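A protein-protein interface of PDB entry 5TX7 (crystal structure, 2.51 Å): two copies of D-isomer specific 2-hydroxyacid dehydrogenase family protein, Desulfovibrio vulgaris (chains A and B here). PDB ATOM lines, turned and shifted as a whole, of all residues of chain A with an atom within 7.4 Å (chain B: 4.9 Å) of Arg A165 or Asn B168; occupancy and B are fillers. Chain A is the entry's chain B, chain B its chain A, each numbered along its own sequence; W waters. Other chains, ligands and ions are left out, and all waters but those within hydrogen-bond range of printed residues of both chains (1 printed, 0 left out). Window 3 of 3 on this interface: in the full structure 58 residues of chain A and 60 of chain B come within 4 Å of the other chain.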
ATOM      1  N   ASP A 101     -27.555  24.431 -25.456  1.00  0.00           N
ATOM      2  CA  ASP A 101     -26.984  23.263 -24.792  1.00  0.00           C
ATOM      3  C   ASP A 101     -25.517  23.040 -25.101  1.00  0.00           C
ATOM      4  O   ASP A 101     -24.767  22.642 -24.203  1.00  0.00           O
ATOM      5  CB  ASP A 101     -27.794  22.027 -25.145  1.00  0.00           C
ATOM      6  CG  ASP A 101     -29.184  22.059 -24.508  1.00  0.00           C
ATOM      7  OD1 ASP A 101     -29.232  22.090 -23.252  1.00  0.00           O
ATOM      8  OD2 ASP A 101     -30.217  22.072 -25.244  1.00  0.00           O
ATOM      9  N   PHE A 108     -19.166  23.754 -18.516  1.00  0.00           N
ATOM     10  CA  PHE A 108     -18.859  22.667 -17.600  1.00  0.00           C
ATOM     11  C   PHE A 108     -17.757  21.723 -18.062  1.00  0.00           C
ATOM     12  O   PHE A 108     -17.062  21.126 -17.208  1.00  0.00           O
ATOM     13  CB  PHE A 108     -20.142  21.931 -17.168  1.00  0.00           C
ATOM     14  CG  PHE A 108     -21.027  22.786 -16.314  1.00  0.00           C
ATOM     15  CD1 PHE A 108     -20.734  22.972 -14.976  1.00  0.00           C
ATOM     16  CD2 PHE A 108     -22.075  23.500 -16.877  1.00  0.00           C
ATOM     17  CE1 PHE A 108     -21.508  23.818 -14.176  1.00  0.00           C
ATOM     18  CE2 PHE A 108     -22.861  24.342 -16.085  1.00  0.00           C
ATOM     19  CZ  PHE A 108     -22.579  24.488 -14.720  1.00  0.00           C
ATOM     20  N   ILE A 153     -23.712  34.049 -12.538  1.00  0.00           N
ATOM     21  CA  ILE A 153     -23.994  34.021 -13.973  1.00  0.00           C
ATOM     22  C   ILE A 153     -24.251  35.456 -14.438  1.00  0.00           C
ATOM     23  O   ILE A 153     -25.251  36.066 -14.060  1.00  0.00           O
ATOM     24  CB  ILE A 153     -25.191  33.099 -14.269  1.00  0.00           C
ATOM     25  CG1 ILE A 153     -24.837  31.676 -13.835  1.00  0.00           C
ATOM     26  CG2 ILE A 153     -25.546  33.113 -15.745  1.00  0.00           C
ATOM     27  CD1 ILE A 153     -25.964  30.683 -13.930  1.00  0.00           C
ATOM     28  N   PHE A 156     -28.438  36.526 -18.202  1.00  0.00           N
ATOM     29  CA  PHE A 156     -29.361  35.432 -17.912  1.00  0.00           C
ATOM     30  C   PHE A 156     -30.364  35.228 -19.041  1.00  0.00           C
ATOM     31  O   PHE A 156     -31.563  35.076 -18.811  1.00  0.00           O
ATOM     32  CB  PHE A 156     -30.029  35.673 -16.549  1.00  0.00           C
ATOM     33  CG  PHE A 156     -30.381  34.419 -15.781  1.00  0.00           C
ATOM     34  CD1 PHE A 156     -29.473  33.375 -15.633  1.00  0.00           C
ATOM     35  CD2 PHE A 156     -31.616  34.315 -15.144  1.00  0.00           C
ATOM     36  CE1 PHE A 156     -29.808  32.242 -14.906  1.00  0.00           C
ATOM     37  CE2 PHE A 156     -31.954  33.190 -14.406  1.00  0.00           C
ATOM     38  CZ  PHE A 156     -31.045  32.157 -14.287  1.00  0.00           C
ATOM     39  N   THR A 159     -28.651  30.634 -22.538  1.00  0.00           N
ATOM     40  CA  THR A 159     -27.449  29.877 -22.221  1.00  0.00           C
ATOM     41  C   THR A 159     -27.163  30.002 -20.730  1.00  0.00           C
ATOM     42  O   THR A 159     -27.000  28.989 -20.051  1.00  0.00           O
ATOM     43  CB  THR A 159     -26.263  30.381 -23.058  1.00  0.00           C
ATOM     44  OG1 THR A 159     -26.565  30.197 -24.441  1.00  0.00           O
ATOM     45  CG2 THR A 159     -25.018  29.611 -22.765  1.00  0.00           C
ATOM     46  N   GLY A 160     -27.119  31.243 -20.236  1.00  0.00           N
ATOM     47  CA  GLY A 160     -27.041  31.538 -18.809  1.00  0.00           C
ATOM     48  C   GLY A 160     -28.007  30.740 -17.971  1.00  0.00           C
ATOM     49  O   GLY A 160     -27.628  30.166 -16.973  1.00  0.00           O
ATOM     50  N   ARG A 161     -29.259  30.683 -18.386  1.00  0.00           N
ATOM     51  CA  ARG A 161     -30.265  29.906 -17.655  1.00  0.00           C
ATOM     52  C   ARG A 161     -29.961  28.424 -17.643  1.00  0.00           C
ATOM     53  O   ARG A 161     -30.182  27.764 -16.636  1.00  0.00           O
ATOM     54  CB  ARG A 161     -31.649  30.106 -18.243  1.00  0.00           C
ATOM     55  CG  ARG A 161     -32.215  31.478 -18.039  1.00  0.00           C
ATOM     56  CD  ARG A 161     -33.342  31.728 -19.031  1.00  0.00           C
ATOM     57  NE  ARG A 161     -33.763  33.121 -19.033  1.00  0.00           N
ATOM     58  CZ  ARG A 161     -34.724  33.618 -19.807  1.00  0.00           C
ATOM     59  NH1 ARG A 161     -35.384  32.826 -20.647  1.00  0.00           N
ATOM     60  NH2 ARG A 161     -35.051  34.911 -19.726  1.00  0.00           N
ATOM     61  N   ARG A 162     -29.484  27.911 -18.782  1.00  0.00           N
ATOM     62  CA  ARG A 162     -29.045  26.518 -18.897  1.00  0.00           C
ATOM     63  C   ARG A 162     -27.851  26.251 -17.978  1.00  0.00           C
ATOM     64  O   ARG A 162     -27.828  25.268 -17.253  1.00  0.00           O
ATOM     65  CB  ARG A 162     -28.715  26.190 -20.346  1.00  0.00           C
ATOM     66  CG  ARG A 162     -28.582  24.692 -20.674  1.00  0.00           C
ATOM     67  CD  ARG A 162     -29.796  23.792 -20.367  1.00  0.00           C
ATOM     68  NE  ARG A 162     -31.127  24.378 -20.645  1.00  0.00           N
ATOM     69  CZ  ARG A 162     -31.914  24.129 -21.700  1.00  0.00           C
ATOM     70  NH1 ARG A 162     -31.537  23.298 -22.664  1.00  0.00           N
ATOM     71  NH2 ARG A 162     -33.088  24.746 -21.797  1.00  0.00           N
ATOM     72  N   VAL A 163     -26.885  27.152 -17.971  1.00  0.00           N
ATOM     73  CA  VAL A 163     -25.765  27.030 -17.043  1.00  0.00           C
ATOM     74  C   VAL A 163     -26.259  26.954 -15.604  1.00  0.00           C
ATOM     75  O   VAL A 163     -25.762  26.147 -14.812  1.00  0.00           O
ATOM     76  CB  VAL A 163     -24.726  28.147 -17.237  1.00  0.00           C
ATOM     77  CG1 VAL A 163     -23.738  28.178 -16.085  1.00  0.00           C
ATOM     78  CG2 VAL A 163     -23.984  27.927 -18.558  1.00  0.00           C
ATOM     79  N   GLY A 164     -27.253  27.773 -15.271  1.00  0.00           N
ATOM     80  CA  GLY A 164     -27.824  27.768 -13.928  1.00  0.00           C
ATOM     81  C   GLY A 164     -28.513  26.469 -13.570  1.00  0.00           C
ATOM     82  O   GLY A 164     -28.346  25.975 -12.471  1.00  0.00           O
ATOM     83  N   ARG A 165     -29.291  25.900 -14.488  1.00  0.00           N
ATOM     84  CA  ARG A 165     -29.953  24.623 -14.206  1.00  0.00           C
ATOM     85  C   ARG A 165     -28.910  23.518 -13.943  1.00  0.00           C
ATOM     86  O   ARG A 165     -29.049  22.733 -12.992  1.00  0.00           O
ATOM     87  CB  ARG A 165     -30.963  24.246 -15.310  1.00  0.00           C
ATOM     88  CG  ARG A 165     -31.381  22.778 -15.332  1.00  0.00           C
ATOM     89  CD  ARG A 165     -32.618  22.516 -16.187  1.00  0.00           C
ATOM     90  NE  ARG A 165     -32.515  21.224 -16.891  1.00  0.00           N
ATOM     91  CZ  ARG A 165     -32.264  21.047 -18.194  1.00  0.00           C
ATOM     92  NH1 ARG A 165     -32.195  19.809 -18.689  1.00  0.00           N
ATOM     93  NH2 ARG A 165     -32.085  22.076 -19.020  1.00  0.00           N
ATOM     94  N   ILE A 166     -27.845  23.495 -14.737  1.00  0.00           N
ATOM     95  CA  ILE A 166     -26.807  22.490 -14.563  1.00  0.00           C
ATOM     96  C   ILE A 166     -26.117  22.686 -13.221  1.00  0.00           C
ATOM     97  O   ILE A 166     -25.977  21.734 -12.438  1.00  0.00           O
ATOM     98  CB  ILE A 166     -25.807  22.506 -15.733  1.00  0.00           C
ATOM     99  CG1 ILE A 166     -26.506  22.058 -17.024  1.00  0.00           C
ATOM    100  CG2 ILE A 166     -24.638  21.577 -15.451  1.00  0.00           C
ATOM    101  CD1 ILE A 166     -25.793  22.455 -18.303  1.00  0.00           C
ATOM    102  N   ALA A 167     -25.725  23.923 -12.944  1.00  0.00           N
ATOM    103  CA  ALA A 167     -25.080  24.280 -11.667  1.00  0.00           C
ATOM    104  C   ALA A 167     -25.897  23.820 -10.461  1.00  0.00           C
ATOM    105  O   ALA A 167     -25.358  23.215  -9.511  1.00  0.00           O
ATOM    106  CB  ALA A 167     -24.858  25.782 -11.582  1.00  0.00           C
ATOM    107  N   ASN A 168     -27.193  24.113 -10.492  1.00  0.00           N
ATOM    108  CA  ASN A 168     -28.083  23.673  -9.432  1.00  0.00           C
ATOM    109  C   ASN A 168     -28.001  22.163  -9.240  1.00  0.00           C
ATOM    110  O   ASN A 168     -27.839  21.690  -8.125  1.00  0.00           O
ATOM    111  CB  ASN A 168     -29.536  24.062  -9.732  1.00  0.00           C
ATOM    112  CG  ASN A 168     -30.506  23.459  -8.735  1.00  0.00           C
ATOM    113  OD1 ASN A 168     -30.608  23.914  -7.573  1.00  0.00           O
ATOM    114  ND2 ASN A 168     -31.207  22.416  -9.165  1.00  0.00           N
ATOM    115  N   ALA A 169     -28.079  21.412 -10.338  1.00  0.00           N
ATOM    116  CA  ALA A 169     -28.050  19.959 -10.271  1.00  0.00           C
ATOM    117  C   ALA A 169     -26.723  19.421  -9.756  1.00  0.00           C
ATOM    118  O   ALA A 169     -26.700  18.370  -9.142  1.00  0.00           O
ATOM    119  CB  ALA A 169     -28.377  19.375 -11.624  1.00  0.00           C
ATOM    120  N   LEU A 170     -25.623  20.135  -9.977  1.00  0.00           N
ATOM    121  CA  LEU A 170     -24.332  19.781  -9.362  1.00  0.00           C
ATOM    122  C   LEU A 170     -24.201  20.181  -7.877  1.00  0.00           C
ATOM    123  O   LEU A 170     -23.111  20.056  -7.303  1.00  0.00           O
ATOM    124  CB  LEU A 170     -23.183  20.416 -10.152  1.00  0.00           C
ATOM    125  CG  LEU A 170     -22.994  19.927 -11.578  1.00  0.00           C
ATOM    126  CD1 LEU A 170     -22.287  21.004 -12.365  1.00  0.00           C
ATOM    127  CD2 LEU A 170     -22.198  18.629 -11.621  1.00  0.00           C
ATOM    128  N   GLY A 171     -25.278  20.672  -7.256  1.00  0.00           N
ATOM    129  CA  GLY A 171     -25.255  21.113  -5.851  1.00  0.00           C
ATOM    130  C   GLY A 171     -24.645  22.476  -5.590  1.00  0.00           C
ATOM    131  O   GLY A 171     -24.208  22.760  -4.465  1.00  0.00           O
ATOM    132  N   VAL A 174     -26.809  29.255  -7.003  1.00  0.00           N
ATOM    133  CA  VAL A 174     -26.805  30.052  -8.219  1.00  0.00           C
ATOM    134  C   VAL A 174     -27.222  31.482  -7.888  1.00  0.00           C
ATOM    135  O   VAL A 174     -28.174  31.708  -7.134  1.00  0.00           O
ATOM    136  CB  VAL A 174     -27.750  29.458  -9.282  1.00  0.00           C
ATOM    137  CG1 VAL A 174     -27.685  30.259 -10.577  1.00  0.00           C
ATOM    138  CG2 VAL A 174     -27.418  27.992  -9.531  1.00  0.00           C
ATOM    139  N   PRO A 185     -36.273  31.125 -12.198  1.00  0.00           N
ATOM    140  CA  PRO A 185     -36.299  29.689 -12.503  1.00  0.00           C
ATOM    141  C   PRO A 185     -36.944  28.878 -11.388  1.00  0.00           C
ATOM    142  O   PRO A 185     -37.173  29.397 -10.286  1.00  0.00           O
ATOM    143  CB  PRO A 185     -34.824  29.334 -12.642  1.00  0.00           C
ATOM    144  CG  PRO A 185     -34.125  30.292 -11.748  1.00  0.00           C
ATOM    145  CD  PRO A 185     -34.944  31.556 -11.727  1.00  0.00           C
ATOM    146  N   TYR A 187     -35.948  26.486  -9.315  1.00  0.00           N
ATOM    147  CA  TYR A 187     -35.004  25.778  -8.450  1.00  0.00           C
ATOM    148  C   TYR A 187     -34.428  26.720  -7.401  1.00  0.00           C
ATOM    149  O   TYR A 187     -34.336  27.927  -7.622  1.00  0.00           O
ATOM    150  CB  TYR A 187     -33.872  25.083  -9.254  1.00  0.00           C
ATOM    151  CG  TYR A 187     -32.995  26.023 -10.064  1.00  0.00           C
ATOM    152  CD1 TYR A 187     -32.012  26.801  -9.455  1.00  0.00           C
ATOM    153  CD2 TYR A 187     -33.134  26.116 -11.450  1.00  0.00           C
ATOM    154  CE1 TYR A 187     -31.215  27.656 -10.200  1.00  0.00           C
ATOM    155  CE2 TYR A 187     -32.330  26.973 -12.197  1.00  0.00           C
ATOM    156  CZ  TYR A 187     -31.383  27.737 -11.556  1.00  0.00           C
ATOM    157  OH  TYR A 187     -30.599  28.586 -12.262  1.00  0.00           O
ATOM    158  N   GLY B 164     -27.356  10.341 -11.943  1.00  0.00           N
ATOM    159  CA  GLY B 164     -28.635  10.451 -12.630  1.00  0.00           C
ATOM    160  C   GLY B 164     -29.216  11.856 -12.592  1.00  0.00           C
ATOM    161  O   GLY B 164     -29.713  12.344 -13.600  1.00  0.00           O
ATOM    162  N   ARG B 165     -29.161  12.517 -11.442  1.00  0.00           N
ATOM    163  CA  ARG B 165     -29.672  13.890 -11.365  1.00  0.00           C
ATOM    164  C   ARG B 165     -28.882  14.823 -12.320  1.00  0.00           C
ATOM    165  O   ARG B 165     -29.468  15.642 -13.041  1.00  0.00           O
ATOM    166  CB  ARG B 165     -29.714  14.422  -9.915  1.00  0.00           C
ATOM    167  N   ILE B 166     -27.568  14.665 -12.359  1.00  0.00           N
ATOM    168  CA  ILE B 166     -26.733  15.499 -13.213  1.00  0.00           C
ATOM    169  C   ILE B 166     -27.072  15.224 -14.674  1.00  0.00           C
ATOM    170  O   ILE B 166     -27.320  16.170 -15.450  1.00  0.00           O
ATOM    171  CB  ILE B 166     -25.234  15.276 -12.929  1.00  0.00           C
ATOM    172  CG1 ILE B 166     -24.897  15.773 -11.517  1.00  0.00           C
ATOM    173  CG2 ILE B 166     -24.383  16.011 -13.951  1.00  0.00           C
ATOM    174  CD1 ILE B 166     -23.591  15.237 -10.952  1.00  0.00           C
ATOM    175  N   ALA B 167     -27.114  13.941 -15.028  1.00  0.00           N
ATOM    176  CA  ALA B 167     -27.478  13.523 -16.391  1.00  0.00           C
ATOM    177  C   ALA B 167     -28.789  14.139 -16.864  1.00  0.00           C
ATOM    178  O   ALA B 167     -28.884  14.677 -17.980  1.00  0.00           O
ATOM    179  CB  ALA B 167     -27.569  11.999 -16.474  1.00  0.00           C
ATOM    180  N   ASN B 168     -29.805  14.045 -16.018  1.00  0.00           N
ATOM    181  CA  ASN B 168     -31.084  14.663 -16.322  1.00  0.00           C
ATOM    182  C   ASN B 168     -30.934  16.149 -16.651  1.00  0.00           C
ATOM    183  O   ASN B 168     -31.443  16.616 -17.658  1.00  0.00           O
ATOM    184  CB  ASN B 168     -32.069  14.490 -15.179  1.00  0.00           C
ATOM    185  CG  ASN B 168     -33.359  15.275 -15.414  1.00  0.00           C
ATOM    186  OD1 ASN B 168     -34.206  14.870 -16.218  1.00  0.00           O
ATOM    187  ND2 ASN B 168     -33.499  16.413 -14.733  1.00  0.00           N
ATOM    188  N   ALA B 169     -30.201  16.873 -15.810  1.00  0.00           N
ATOM    189  CA  ALA B 169     -30.018  18.307 -16.000  1.00  0.00           C
ATOM    190  C   ALA B 169     -29.257  18.645 -17.283  1.00  0.00           C
ATOM    191  O   ALA B 169     -29.479  19.686 -17.870  1.00  0.00           O
ATOM    192  CB  ALA B 169     -29.319  18.901 -14.805  1.00  0.00           C
ATOM    193  N   LEU B 170     -28.373  17.755 -17.732  1.00  0.00           N
ATOM    194  CA  LEU B 170     -27.720  17.913 -19.032  1.00  0.00           C
ATOM    195  C   LEU B 170     -28.603  17.486 -20.233  1.00  0.00           C
ATOM    196  O   LEU B 170     -28.097  17.366 -21.347  1.00  0.00           O
ATOM    197  CB  LEU B 170     -26.414  17.108 -19.059  1.00  0.00           C
ATOM    198  CG  LEU B 170     -25.324  17.569 -18.106  1.00  0.00           C
ATOM    199  CD1 LEU B 170     -24.405  16.404 -17.829  1.00  0.00           C
ATOM    200  CD2 LEU B 170     -24.536  18.755 -18.643  1.00  0.00           C
ATOM    201  N   GLY B 171     -29.889  17.217 -20.015  1.00  0.00           N
ATOM    202  CA  GLY B 171     -30.802  16.792 -21.087  1.00  0.00           C
ATOM    203  C   GLY B 171     -30.732  15.333 -21.516  1.00  0.00           C
ATOM    204  O   GLY B 171     -31.203  15.004 -22.593  1.00  0.00           O
ATOM    205  N   MET B 172     -30.154  14.464 -20.686  1.00  0.00           N
ATOM    206  CA  MET B 172     -30.059  13.043 -20.998  1.00  0.00           C
ATOM    207  C   MET B 172     -31.264  12.301 -20.423  1.00  0.00           C
ATOM    208  O   MET B 172     -31.820  12.691 -19.400  1.00  0.00           O
ATOM    209  CB  MET B 172     -28.785  12.418 -20.418  1.00  0.00           C
ATOM    210  CG  MET B 172     -27.501  13.115 -20.774  1.00  0.00           C
ATOM    211  SD  MET B 172     -26.004  12.372 -20.097  1.00  0.00           S
ATOM    212  CE  MET B 172     -25.884  10.979 -21.229  1.00  0.00           C
ATOM    213  N   VAL B 174     -32.375   8.928 -18.532  1.00  0.00           N
ATOM    214  CA  VAL B 174     -31.717   8.120 -17.520  1.00  0.00           C
ATOM    215  C   VAL B 174     -32.435   6.774 -17.404  1.00  0.00           C
ATOM    216  O   VAL B 174     -33.661   6.704 -17.376  1.00  0.00           O
ATOM    217  CB  VAL B 174     -31.701   8.827 -16.157  1.00  0.00           C
ATOM    218  CG1 VAL B 174     -30.959   8.006 -15.124  1.00  0.00           C
ATOM    219  CG2 VAL B 174     -31.070  10.210 -16.285  1.00  0.00           C
ATOM    220  N   TYR B 187     -37.558  13.094 -11.346  1.00  0.00           N
ATOM    221  CA  TYR B 187     -37.270  13.662 -12.670  1.00  0.00           C
ATOM    222  C   TYR B 187     -37.611  12.656 -13.762  1.00  0.00           C
ATOM    223  O   TYR B 187     -37.580  11.444 -13.544  1.00  0.00           O
ATOM    224  CB  TYR B 187     -35.814  14.146 -12.798  1.00  0.00           C
ATOM    225  CG  TYR B 187     -34.757  13.065 -12.628  1.00  0.00           C
ATOM    226  CD1 TYR B 187     -34.483  12.161 -13.648  1.00  0.00           C
ATOM    227  CD2 TYR B 187     -34.028  12.946 -11.433  1.00  0.00           C
ATOM    228  CE1 TYR B 187     -33.545  11.160 -13.484  1.00  0.00           C
ATOM    229  CE2 TYR B 187     -33.077  11.957 -11.275  1.00  0.00           C
ATOM    230  CZ  TYR B 187     -32.844  11.068 -12.308  1.00  0.00           C
ATOM    231  OH  TYR B 187     -31.922  10.096 -12.159  1.00  0.00           O
ATOM    232  N   ARG B 188     -37.923  13.171 -14.942  1.00  0.00           N
ATOM    233  CA  ARG B 188     -38.214  12.346 -16.098  1.00  0.00           C
ATOM    234  C   ARG B 188     -37.491  12.923 -17.313  1.00  0.00           C
ATOM    235  O   ARG B 188     -37.209  14.113 -17.326  1.00  0.00           O
ATOM    236  CB  ARG B 188     -39.728  12.311 -16.311  1.00  0.00           C
ATOM    237  CG  ARG B 188     -40.499  11.624 -15.185  1.00  0.00           C
ATOM    238  CD  ARG B 188     -40.122  10.145 -15.036  1.00  0.00           C
ATOM    239  NE  ARG B 188     -40.946   9.472 -14.036  1.00  0.00           N
ATOM    240  CZ  ARG B 188     -40.631   9.259 -12.754  1.00  0.00           C
ATOM    241  NH1 ARG B 188     -39.470   9.663 -12.216  1.00  0.00           N
ATOM    242  NH2 ARG B 188     -41.526   8.626 -11.984  1.00  0.00           N
ATOM    243  N   PRO B 189     -37.159  12.117 -18.322  1.00  0.00           N
ATOM    244  CA  PRO B 189     -37.443  10.670 -18.396  1.00  0.00           C
ATOM    245  C   PRO B 189     -36.509   9.823 -17.537  1.00  0.00           C
ATOM    246  O   PRO B 189     -35.295  10.026 -17.551  1.00  0.00           O
ATOM    247  CB  PRO B 189     -37.207  10.339 -19.886  1.00  0.00           C
ATOM    248  CG  PRO B 189     -37.174  11.674 -20.568  1.00  0.00           C
ATOM    249  CD  PRO B 189     -36.539  12.584 -19.569  1.00  0.00           C
HETATM  250  O   HOH W   1     -27.641  20.788 -21.387  1.00  0.00           O
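The side-chain amide oxygen (OD1) of Asn B168 lies close to the backbone carbonyl oxygen (O) of Arg B188 (3.3 Å).
Of the 20 printed residues of chain A, 4 touch a printed residue of chain B.
Printed residues of chain A that touch a printed residue of chain B: Arg A165, Ile A166, Ala A169 and Leu A170.
Printed residues of chain B that touch a printed residue of chain A: Ile B166, Asn B168, Ala B169, Leu B170 and Gly B171.
Hydrophobic or aromatic side chains of chain B within 4 Å of the printed part of chain A: Ile B166, Ala B169 and Leu B170.
Among the printed residues, 8 pairs touch across the chains.
Among the printed residues, no Asp or Glu carboxylate lies within 4 Å of a Lys or Arg side-chain nitrogen of the other chain.
Water W1 bridges OD1 of Asp A101 (2.8 Å) and O of Leu B170 (3.5 Å).
O of Asn B168 sits at hydrogen-bond distance from NH1 of Arg A165.
The guanidinium group of Arg A165 sits at hydrogen-bond distance from the backbone carbonyl oxygen of Ala B169 (2.8 Å).
Arg A165 touches Asn B168, but with the chains exchanged Asn A168 does not touch Arg B165 (7.7 Å).
Arg A165 touches Ala B169, but with the chains exchanged Ala A169 does not touch Arg B165 (4.1 Å).
Ile A166 touches Ala B169, and with the chains exchanged Ala A169 touches Ile B166.
Ile A166 touches Leu B170, and with the chains exchanged Leu A170 touches Ile B166.
Arg A165 touches Gly B171 (NH1 to N, 3.7 Å).
Ile A166 touches Ala B169 (CG1 to O, 3.9 Å).
Ile A166 touches Leu B170.
Ile B166 touches Ala A169 (CG1 to O, 3.95 Å).
Ala B169 touches Ala A169 (CB to CB, 3.4 Å).
CD2 of Leu A170 touches CD1 of Ile B166, 3.7 Å away.
Arg A165 touches three residues of chain B.
Asn B168 touches just one residue of chain A: Arg A165 (3.4 Å).
Ala B167 touches none of the printed residues of chain A.
Of the printed residues of chain A, Leu B170 touches Ile A166 (3.9 Å).
Printed residues of chain A within 4 Å of Gly B171: Arg A165 (3.7 Å).
Tyr A187 touches none of the printed residues of chain B.
The nearest residue of chain B that does not touch Arg A165 is Leu B170 (4.4 Å).
The nearest printed residue of chain A that does not touch Gly B171 is Asp A101 (5.9 Å).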
